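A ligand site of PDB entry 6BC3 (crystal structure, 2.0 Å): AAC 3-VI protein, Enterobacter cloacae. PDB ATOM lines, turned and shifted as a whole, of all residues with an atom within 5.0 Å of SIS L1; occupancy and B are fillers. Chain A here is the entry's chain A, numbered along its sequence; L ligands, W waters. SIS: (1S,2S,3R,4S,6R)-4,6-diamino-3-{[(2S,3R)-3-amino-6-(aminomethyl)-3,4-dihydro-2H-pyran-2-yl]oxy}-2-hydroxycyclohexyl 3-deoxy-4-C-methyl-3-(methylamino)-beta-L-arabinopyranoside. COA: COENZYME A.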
ATOM      1  N   PHE A  80     -25.764   9.465  11.880  1.00  0.00           N
ATOM      2  CA  PHE A  80     -24.971   9.620  13.089  1.00  0.00           C
ATOM      3  C   PHE A  80     -24.109  10.866  12.926  1.00  0.00           C
ATOM      4  O   PHE A  80     -23.084  10.849  12.242  1.00  0.00           O
ATOM      5  CB  PHE A  80     -24.119   8.378  13.347  1.00  0.00           C
ATOM      6  CG  PHE A  80     -23.147   8.534  14.481  1.00  0.00           C
ATOM      7  CD1 PHE A  80     -21.857   8.024  14.374  1.00  0.00           C
ATOM      8  CD2 PHE A  80     -23.502   9.185  15.649  1.00  0.00           C
ATOM      9  CE1 PHE A  80     -20.951   8.152  15.417  1.00  0.00           C
ATOM     10  CE2 PHE A  80     -22.602   9.325  16.687  1.00  0.00           C
ATOM     11  CZ  PHE A  80     -21.324   8.814  16.572  1.00  0.00           C
ATOM     12  N   SER A  82     -23.351  13.110  15.800  1.00  0.00           N
ATOM     13  CA  SER A  82     -22.581  13.324  17.039  1.00  0.00           C
ATOM     14  C   SER A  82     -22.570  14.822  17.341  1.00  0.00           C
ATOM     15  O   SER A  82     -23.580  15.514  17.088  1.00  0.00           O
ATOM     16  CB  SER A  82     -21.212  12.682  16.903  1.00  0.00           C
ATOM     17  OG  SER A  82     -20.478  12.799  18.116  1.00  0.00           O
ATOM     18  N   TRP A  83     -21.474  15.357  17.859  1.00  0.00           N
ATOM     19  CA  TRP A  83     -21.397  16.747  18.288  1.00  0.00           C
ATOM     20  C   TRP A  83     -19.958  17.215  18.143  1.00  0.00           C
ATOM     21  O   TRP A  83     -19.032  16.508  18.549  1.00  0.00           O
ATOM     22  CB  TRP A  83     -21.861  16.894  19.742  1.00  0.00           C
ATOM     23  CG  TRP A  83     -21.811  18.285  20.313  1.00  0.00           C
ATOM     24  CD1 TRP A  83     -21.779  19.457  19.628  1.00  0.00           C
ATOM     25  CD2 TRP A  83     -21.790  18.632  21.696  1.00  0.00           C
ATOM     26  NE1 TRP A  83     -21.730  20.521  20.497  1.00  0.00           N
ATOM     27  CE2 TRP A  83     -21.745  20.042  21.776  1.00  0.00           C
ATOM     28  CE3 TRP A  83     -21.807  17.889  22.886  1.00  0.00           C
ATOM     29  CZ2 TRP A  83     -21.719  20.721  22.996  1.00  0.00           C
ATOM     30  CZ3 TRP A  83     -21.780  18.563  24.092  1.00  0.00           C
ATOM     31  CH2 TRP A  83     -21.725  19.967  24.144  1.00  0.00           C
ATOM     32  N   SER A  86     -18.170  17.597  21.685  1.00  0.00           N
ATOM     33  CA  SER A  86     -18.456  16.563  22.679  1.00  0.00           C
ATOM     34  C   SER A  86     -17.264  16.395  23.611  1.00  0.00           C
ATOM     35  O   SER A  86     -16.145  16.162  23.150  1.00  0.00           O
ATOM     36  CB  SER A  86     -18.772  15.234  21.989  1.00  0.00           C
ATOM     37  OG  SER A  86     -18.918  14.194  22.937  1.00  0.00           O
ATOM     38  N   TYR A  88     -15.808  14.112  25.146  1.00  0.00           N
ATOM     39  CA  TYR A  88     -15.557  12.681  25.314  1.00  0.00           C
ATOM     40  C   TYR A  88     -14.200  12.435  25.966  1.00  0.00           C
ATOM     41  O   TYR A  88     -14.117  11.882  27.064  1.00  0.00           O
ATOM     42  CB  TYR A  88     -15.648  11.984  23.962  1.00  0.00           C
ATOM     43  CG  TYR A  88     -15.591  10.467  24.034  1.00  0.00           C
ATOM     44  CD1 TYR A  88     -16.735   9.719  24.283  1.00  0.00           C
ATOM     45  CD2 TYR A  88     -14.401   9.791  23.849  1.00  0.00           C
ATOM     46  CE1 TYR A  88     -16.698   8.341  24.346  1.00  0.00           C
ATOM     47  CE2 TYR A  88     -14.341   8.409  23.915  1.00  0.00           C
ATOM     48  CZ  TYR A  88     -15.496   7.685  24.155  1.00  0.00           C
ATOM     49  OH  TYR A  88     -15.441   6.315  24.216  1.00  0.00           O
ATOM     50  N   GLU A  89     -13.115  12.849  25.295  1.00  0.00           N
ATOM     51  CA  GLU A  89     -11.788  12.645  25.861  1.00  0.00           C
ATOM     52  C   GLU A  89     -11.578  13.468  27.124  1.00  0.00           C
ATOM     53  O   GLU A  89     -10.831  13.052  28.018  1.00  0.00           O
ATOM     54  CB  GLU A  89     -10.712  13.006  24.839  1.00  0.00           C
ATOM     55  CG  GLU A  89     -10.761  12.186  23.551  1.00  0.00           C
ATOM     56  CD  GLU A  89     -11.437  12.939  22.419  1.00  0.00           C
ATOM     57  OE1 GLU A  89     -12.292  13.805  22.697  1.00  0.00           O
ATOM     58  OE2 GLU A  89     -11.102  12.667  21.234  1.00  0.00           O
ATOM     59  N   TYR A 116     -20.256  16.600  14.450  1.00  0.00           N
ATOM     60  CA  TYR A 116     -18.829  16.319  14.489  1.00  0.00           C
ATOM     61  C   TYR A 116     -18.277  16.258  13.075  1.00  0.00           C
ATOM     62  O   TYR A 116     -18.695  15.397  12.294  1.00  0.00           O
ATOM     63  CB  TYR A 116     -18.559  15.006  15.219  1.00  0.00           C
ATOM     64  CG  TYR A 116     -17.095  14.723  15.457  1.00  0.00           C
ATOM     65  CD1 TYR A 116     -16.393  15.405  16.440  1.00  0.00           C
ATOM     66  CD2 TYR A 116     -16.411  13.781  14.701  1.00  0.00           C
ATOM     67  CE1 TYR A 116     -15.046  15.156  16.660  1.00  0.00           C
ATOM     68  CE2 TYR A 116     -15.073  13.523  14.910  1.00  0.00           C
ATOM     69  CZ  TYR A 116     -14.398  14.217  15.894  1.00  0.00           C
ATOM     70  OH  TYR A 116     -13.055  13.977  16.119  1.00  0.00           O
ATOM     71  N   PHE A 119     -16.989  12.878  11.083  1.00  0.00           N
ATOM     72  CA  PHE A 119     -17.889  11.848  10.595  1.00  0.00           C
ATOM     73  C   PHE A 119     -18.547  12.215   9.277  1.00  0.00           C
ATOM     74  O   PHE A 119     -19.487  11.532   8.845  1.00  0.00           O
ATOM     75  CB  PHE A 119     -18.954  11.522  11.650  1.00  0.00           C
ATOM     76  CG  PHE A 119     -18.388  11.039  12.962  1.00  0.00           C
ATOM     77  CD1 PHE A 119     -17.168  10.383  12.999  1.00  0.00           C
ATOM     78  CD2 PHE A 119     -19.072  11.249  14.140  1.00  0.00           C
ATOM     79  CE1 PHE A 119     -16.643   9.932  14.192  1.00  0.00           C
ATOM     80  CE2 PHE A 119     -18.557  10.799  15.347  1.00  0.00           C
ATOM     81  CZ  PHE A 119     -17.340  10.147  15.375  1.00  0.00           C
ATOM     82  N   ASP A 139     -22.861  12.707  22.628  1.00  0.00           N
ATOM     83  CA  ASP A 139     -21.754  12.087  21.912  1.00  0.00           C
ATOM     84  C   ASP A 139     -22.227  11.176  20.784  1.00  0.00           C
ATOM     85  O   ASP A 139     -21.586  11.121  19.735  1.00  0.00           O
ATOM     86  CB  ASP A 139     -20.869  11.293  22.887  1.00  0.00           C
ATOM     87  CG  ASP A 139     -19.575  10.840  22.245  1.00  0.00           C
ATOM     88  OD1 ASP A 139     -18.704  11.698  21.986  1.00  0.00           O
ATOM     89  OD2 ASP A 139     -19.429   9.621  22.002  1.00  0.00           O
ATOM     90  N   TYR A 162     -25.562   3.034  21.143  1.00  0.00           N
ATOM     91  CA  TYR A 162     -25.785   2.361  19.875  1.00  0.00           C
ATOM     92  C   TYR A 162     -26.427   0.989  20.012  1.00  0.00           C
ATOM     93  O   TYR A 162     -26.672   0.333  18.979  1.00  0.00           O
ATOM     94  CB  TYR A 162     -24.457   2.215  19.117  1.00  0.00           C
ATOM     95  CG  TYR A 162     -23.628   3.480  19.104  1.00  0.00           C
ATOM     96  CD1 TYR A 162     -22.521   3.615  19.933  1.00  0.00           C
ATOM     97  CD2 TYR A 162     -23.964   4.543  18.277  1.00  0.00           C
ATOM     98  CE1 TYR A 162     -21.764   4.773  19.934  1.00  0.00           C
ATOM     99  CE2 TYR A 162     -23.209   5.705  18.269  1.00  0.00           C
ATOM    100  CZ  TYR A 162     -22.113   5.815  19.092  1.00  0.00           C
ATOM    101  OH  TYR A 162     -21.365   6.969  19.095  1.00  0.00           O
ATOM    102  N   ASP A 186     -15.238   0.824   7.620  1.00  0.00           N
ATOM    103  CA  ASP A 186     -15.212   1.214   9.017  1.00  0.00           C
ATOM    104  C   ASP A 186     -16.367   2.137   9.397  1.00  0.00           C
ATOM    105  O   ASP A 186     -16.611   2.333  10.591  1.00  0.00           O
ATOM    106  CB  ASP A 186     -13.894   1.914   9.353  1.00  0.00           C
ATOM    107  CG  ASP A 186     -13.756   3.262   8.658  1.00  0.00           C
ATOM    108  OD1 ASP A 186     -13.684   3.286   7.411  1.00  0.00           O
ATOM    109  OD2 ASP A 186     -13.748   4.298   9.363  1.00  0.00           O
ATOM    110  N   ALA A 187     -17.077   2.691   8.422  1.00  0.00           N
ATOM    111  CA  ALA A 187     -18.096   3.698   8.692  1.00  0.00           C
ATOM    112  C   ALA A 187     -19.443   3.097   9.081  1.00  0.00           C
ATOM    113  O   ALA A 187     -20.348   3.859   9.457  1.00  0.00           O
ATOM    114  CB  ALA A 187     -18.278   4.605   7.469  1.00  0.00           C
ATOM    115  N   HIS A 192     -22.218  -1.223  15.636  1.00  0.00           N
ATOM    116  CA  HIS A 192     -22.015  -1.091  17.071  1.00  0.00           C
ATOM    117  C   HIS A 192     -23.148  -1.706  17.868  1.00  0.00           C
ATOM    118  O   HIS A 192     -22.959  -2.031  19.044  1.00  0.00           O
ATOM    119  CB  HIS A 192     -21.850   0.382  17.450  1.00  0.00           C
ATOM    120  CG  HIS A 192     -20.567   0.981  16.990  1.00  0.00           C
ATOM    121  ND1 HIS A 192     -19.341   0.408  17.268  1.00  0.00           N
ATOM    122  CD2 HIS A 192     -20.307   2.104  16.272  1.00  0.00           C
ATOM    123  CE1 HIS A 192     -18.387   1.150  16.739  1.00  0.00           C
ATOM    124  NE2 HIS A 192     -18.945   2.182  16.134  1.00  0.00           N
ATOM    125  N   SER A 228     -17.115   2.364  21.768  1.00  0.00           N
ATOM    126  CA  SER A 228     -17.407   2.502  20.341  1.00  0.00           C
ATOM    127  C   SER A 228     -16.144   2.570  19.484  1.00  0.00           C
ATOM    128  O   SER A 228     -16.252   2.654  18.258  1.00  0.00           O
ATOM    129  CB  SER A 228     -18.274   3.732  20.094  1.00  0.00           C
ATOM    130  OG  SER A 228     -17.580   4.924  20.405  1.00  0.00           O
ATOM    131  N   ASN A 229     -14.972   2.552  20.101  1.00  0.00           N
ATOM    132  CA  ASN A 229     -13.701   2.494  19.383  1.00  0.00           C
ATOM    133  C   ASN A 229     -13.106   1.084  19.376  1.00  0.00           C
ATOM    134  O   ASN A 229     -11.896   0.929  19.207  1.00  0.00           O
ATOM    135  CB  ASN A 229     -12.708   3.476  19.991  1.00  0.00           C
ATOM    136  CG  ASN A 229     -13.014   4.920  19.612  1.00  0.00           C
ATOM    137  OD1 ASN A 229     -13.170   5.245  18.437  1.00  0.00           O
ATOM    138  ND2 ASN A 229     -13.100   5.783  20.613  1.00  0.00           N
ATOM    139  N   GLY A 230     -13.947   0.064  19.553  1.00  0.00           N
ATOM    140  CA  GLY A 230     -13.473  -1.306  19.609  1.00  0.00           C
ATOM    141  C   GLY A 230     -14.092  -2.075  20.760  1.00  0.00           C
ATOM    142  O   GLY A 230     -13.890  -1.725  21.923  1.00  0.00           O
ATOM    143  N   GLY A 240      -4.648  -0.299  13.052  1.00  0.00           N
ATOM    144  CA  GLY A 240      -5.862  -0.248  13.850  1.00  0.00           C
ATOM    145  C   GLY A 240      -7.229  -0.443  13.199  1.00  0.00           C
ATOM    146  O   GLY A 240      -8.123   0.374  13.426  1.00  0.00           O
ATOM    147  N   ASP A 242     -10.770  -1.709  13.354  1.00  0.00           N
ATOM    148  CA  ASP A 242     -11.617  -2.081  14.480  1.00  0.00           C
ATOM    149  C   ASP A 242     -12.531  -3.243  14.102  1.00  0.00           C
ATOM    150  O   ASP A 242     -12.461  -3.786  12.994  1.00  0.00           O
ATOM    151  CB  ASP A 242     -12.408  -0.861  14.952  1.00  0.00           C
ATOM    152  CG  ASP A 242     -13.229  -0.218  13.855  1.00  0.00           C
ATOM    153  OD1 ASP A 242     -13.968   0.741  14.156  1.00  0.00           O
ATOM    154  OD2 ASP A 242     -13.154  -0.688  12.697  1.00  0.00           O
HETATM  155  C11 SIS L   1     -13.834   5.772  14.045  1.00  0.00           C
HETATM  156  C12 SIS L   1     -17.682   6.721  17.463  1.00  0.00           C
HETATM  157  C13 SIS L   1     -15.845   8.404  19.530  1.00  0.00           C
HETATM  158  C21 SIS L   1     -13.661   5.851  12.744  1.00  0.00           C
HETATM  159  C22 SIS L   1     -17.795   5.272  16.888  1.00  0.00           C
HETATM  160  C23 SIS L   1     -16.506   9.663  20.121  1.00  0.00           C
HETATM  161  C31 SIS L   1     -12.092   5.591  12.258  1.00  0.00           C
HETATM  162  C32 SIS L   1     -17.148   5.214  15.447  1.00  0.00           C
HETATM  163  C33 SIS L   1     -15.985  10.871  19.412  1.00  0.00           C
HETATM  164  C41 SIS L   1     -11.488   4.531  12.861  1.00  0.00           C
HETATM  165  C42 SIS L   1     -15.659   5.653  15.586  1.00  0.00           C
HETATM  166  C43 SIS L   1     -14.500  10.968  19.523  1.00  0.00           C
HETATM  167  C51 SIS L   1     -11.996   4.136  14.299  1.00  0.00           C
HETATM  168  C52 SIS L   1     -15.417   6.909  16.482  1.00  0.00           C
HETATM  169  C53 SIS L   1     -13.790   9.667  19.078  1.00  0.00           C
HETATM  170  C61 SIS L   1     -11.075   3.506  15.282  1.00  0.00           C
HETATM  171  C62 SIS L   1     -16.259   7.025  17.727  1.00  0.00           C
HETATM  172  C83 SIS L   1     -13.968  12.121  18.623  1.00  0.00           C
HETATM  173  C93 SIS L   1     -17.432  12.806  19.032  1.00  0.00           C
HETATM  174  N12 SIS L   1     -18.511   6.871  18.672  1.00  0.00           N
HETATM  175  N21 SIS L   1     -14.556   4.856  12.000  1.00  0.00           N
HETATM  176  N32 SIS L   1     -17.196   3.914  14.954  1.00  0.00           N
HETATM  177  N33 SIS L   1     -16.637  12.094  20.033  1.00  0.00           N
HETATM  178  N61 SIS L   1     -11.781   2.909  16.447  1.00  0.00           N
HETATM  179  O11 SIS L   1     -15.266   5.925  14.281  1.00  0.00           O
HETATM  180  O23 SIS L   1     -17.913   9.565  19.931  1.00  0.00           O
HETATM  181  O43 SIS L   1     -14.151  11.243  20.879  1.00  0.00           O
HETATM  182  O51 SIS L   1     -13.335   4.384  14.654  1.00  0.00           O
HETATM  183  O52 SIS L   1     -14.053   6.963  16.869  1.00  0.00           O
HETATM  184  O53 SIS L   1     -14.373   8.447  19.690  1.00  0.00           O
HETATM  185  O62 SIS L   1     -16.151   8.411  18.212  1.00  0.00           O
HETATM  186  N1A COA L   2     -19.713  23.754   2.378  1.00  0.00           N
HETATM  187  C2A COA L   2     -19.026  23.297   1.295  1.00  0.00           C
HETATM  188  N3A COA L   2     -18.035  22.371   1.431  1.00  0.00           N
HETATM  189  C4A COA L   2     -17.729  21.881   2.675  1.00  0.00           C
HETATM  190  C5A COA L   2     -18.403  22.329   3.740  1.00  0.00           C
HETATM  191  C6A COA L   2     -19.411  23.285   3.576  1.00  0.00           C
HETATM  192  N6A COA L   2     -20.267  23.908   4.529  1.00  0.00           N
HETATM  193  N7A COA L   2     -17.927  21.716   4.841  1.00  0.00           N
HETATM  194  C8A COA L   2     -16.953  20.891   4.432  1.00  0.00           C
HETATM  195  N9A COA L   2     -16.834  20.983   3.107  1.00  0.00           N
HETATM  196  C1B COA L   2     -15.921  20.286   2.253  1.00  0.00           C
HETATM  197  C2B COA L   2     -14.796  20.114   2.904  1.00  0.00           C
HETATM  198  O2B COA L   2     -14.108  21.357   3.015  1.00  0.00           O
HETATM  199  C3B COA L   2     -14.102  19.123   1.971  1.00  0.00           C
HETATM  200  O3B COA L   2     -13.857  19.710   0.797  1.00  0.00           O
HETATM  201  P3B COA L   2     -12.279  20.236   0.476  1.00  0.00           P
HETATM  202  O7A COA L   2     -11.294  19.199   0.950  1.00  0.00           O
HETATM  203  O8A COA L   2     -12.020  21.575   1.198  1.00  0.00           O
HETATM  204  O9A COA L   2     -12.126  20.424  -1.012  1.00  0.00           O
HETATM  205  C4B COA L   2     -15.252  18.075   1.797  1.00  0.00           C
HETATM  206  O4B COA L   2     -16.371  18.751   1.848  1.00  0.00           O
HETATM  207  C5B COA L   2     -15.203  17.106   2.969  1.00  0.00           C
HETATM  208  O5B COA L   2     -15.921  15.943   2.653  1.00  0.00           O
HETATM  209  P1A COA L   2     -16.090  14.806   3.850  1.00  0.00           P
HETATM  210  O1A COA L   2     -16.534  15.488   5.123  1.00  0.00           O
HETATM  211  O2A COA L   2     -17.176  13.841   3.443  1.00  0.00           O
HETATM  212  O3A COA L   2     -14.644  14.028   4.094  1.00  0.00           O
HETATM  213  P2A COA L   2     -13.975  12.993   2.896  1.00  0.00           P
HETATM  214  O4A COA L   2     -12.487  13.309   2.688  1.00  0.00           O
HETATM  215  O5A COA L   2     -14.690  13.166   1.565  1.00  0.00           O
HETATM  216  O6A COA L   2     -14.099  11.421   3.434  1.00  0.00           O
HETATM  217  CBP COA L   2     -14.850  10.588   5.557  1.00  0.00           C
HETATM  218  CCP COA L   2     -13.688  11.187   4.767  1.00  0.00           C
HETATM  219  CDP COA L   2     -15.862  11.634   5.851  1.00  0.00           C
HETATM  220  CEP COA L   2     -14.348  10.052   6.880  1.00  0.00           C
HETATM  221  CAP COA L   2     -15.461   9.430   4.722  1.00  0.00           C
HETATM  222  OAP COA L   2     -14.458   8.646   4.252  1.00  0.00           O
HETATM  223  C9P COA L   2     -16.408   8.579   5.617  1.00  0.00           C
HETATM  224  O9P COA L   2     -16.016   7.531   6.077  1.00  0.00           O
HETATM  225  N8P COA L   2     -17.790   9.101   5.912  1.00  0.00           N
HETATM  226  C7P COA L   2     -18.698   8.292   6.824  1.00  0.00           C
HETATM  227  C6P COA L   2     -18.145   8.548   8.234  1.00  0.00           C
HETATM  228  C5P COA L   2     -19.157   8.169   9.341  1.00  0.00           C
HETATM  229  O5P COA L   2     -20.319   8.109   9.124  1.00  0.00           O
HETATM  230  N4P COA L   2     -18.669   7.925  10.635  1.00  0.00           N
HETATM  231  C3P COA L   2     -19.589   7.573  11.691  1.00  0.00           C
HETATM  232  C2P COA L   2     -18.709   6.868  12.768  1.00  0.00           C
HETATM  233  S1P COA L   2     -18.147   5.275  12.035  1.00  0.00           S
HETATM  234  O   HOH W   1     -15.390  14.579  21.126  1.00  0.00           O
HETATM  235  O   HOH W   2     -15.698   2.498  13.103  1.00  0.00           O
HETATM  236  O   HOH W   3     -15.826   7.564  10.660  1.00  0.00           O
HETATM  237  O   HOH W   4     -12.925   9.131  15.163  1.00  0.00           O
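Water W2 lies within hydrogen-bond range of O of Asp 186 (2.7 Å), OD1 of Asp 242 (2.7 Å) and N32 of SIS L1 (2.8 Å).
Water W1 bridges the backbone carbonyl oxygen (O) of Ser 86 (2.7 Å) and a nitrogen (N33) of SIS L1 (3.0 Å).
Water W3 lies within hydrogen-bond range of N4P of COA L2 (2.9 Å) and N21 of SIS L1 (3.3 Å).
Merely in contact with SIS L1: Ser 82 (3.2 Å), Tyr 88 (3.3 Å), Tyr 116 (3.2 Å) and Phe 119 (3.5 Å).
The nearest printed residue that does not touch SIS L1 is Phe 80 (4.01 Å).
A nitrogen (N32) of SIS L1 lies close to a sulfur (S1P) of COA L2, 3.4 Å away.
The side-chain carboxylate (OE2) of Glu 89 lies within hydrogen-bond range of an oxygen (O43) of SIS L1, 3.4 Å away.
OD1 of Asn 229 lies within hydrogen-bond range of O52 of SIS L1, 2.5 Å away.
A ring nitrogen (NE2) of His 192 lies within hydrogen-bond range of a nitrogen (N32) of SIS L1 (2.7 Å).
OD1 of Asp 139 lies within salt-bridge range of N33 of SIS L1, 2.9 Å away.
The backbone carbonyl oxygen (O) of Asp 186 sits close to a sulfur (S1P) of COA L2 (3.6 Å).
A nitrogen (N12) of SIS L1 is in hydrogen-bond range of the side-chain hydroxyl (OG) of Ser 228, 2.8 Å away.
The side-chain carboxylate (OD2) of Asp 186 is in salt-bridge range of a nitrogen (N21) of SIS L1, 2.8 Å away.
O of Ala 187 lies close to S1P of COA L2 (3.7 Å).
The side-chain hydroxyl (OH) of Tyr 162 is in hydrogen-bond range of a nitrogen (N12) of SIS L1 (2.9 Å).
OD1 of Asp 242 is in salt-bridge range of N61 of SIS L1 (3.8 Å).
O of Asn 229 lies within hydrogen-bond range of N61 of SIS L1 (3.4 Å).
The backbone carbonyl oxygen (O) of Asp 139 sits at hydrogen-bond distance from the side-chain hydroxyl (OG) of Ser 82, at 2.6 Å.
A ring nitrogen (NE2) of His 192 lies close to the backbone carbonyl oxygen (O) of Ser 228.
The side-chain hydroxyl (OG) of Ser 86 is in hydrogen-bond range of the side-chain carboxylate (OD1) of Asp 139, 2.7 Å away.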
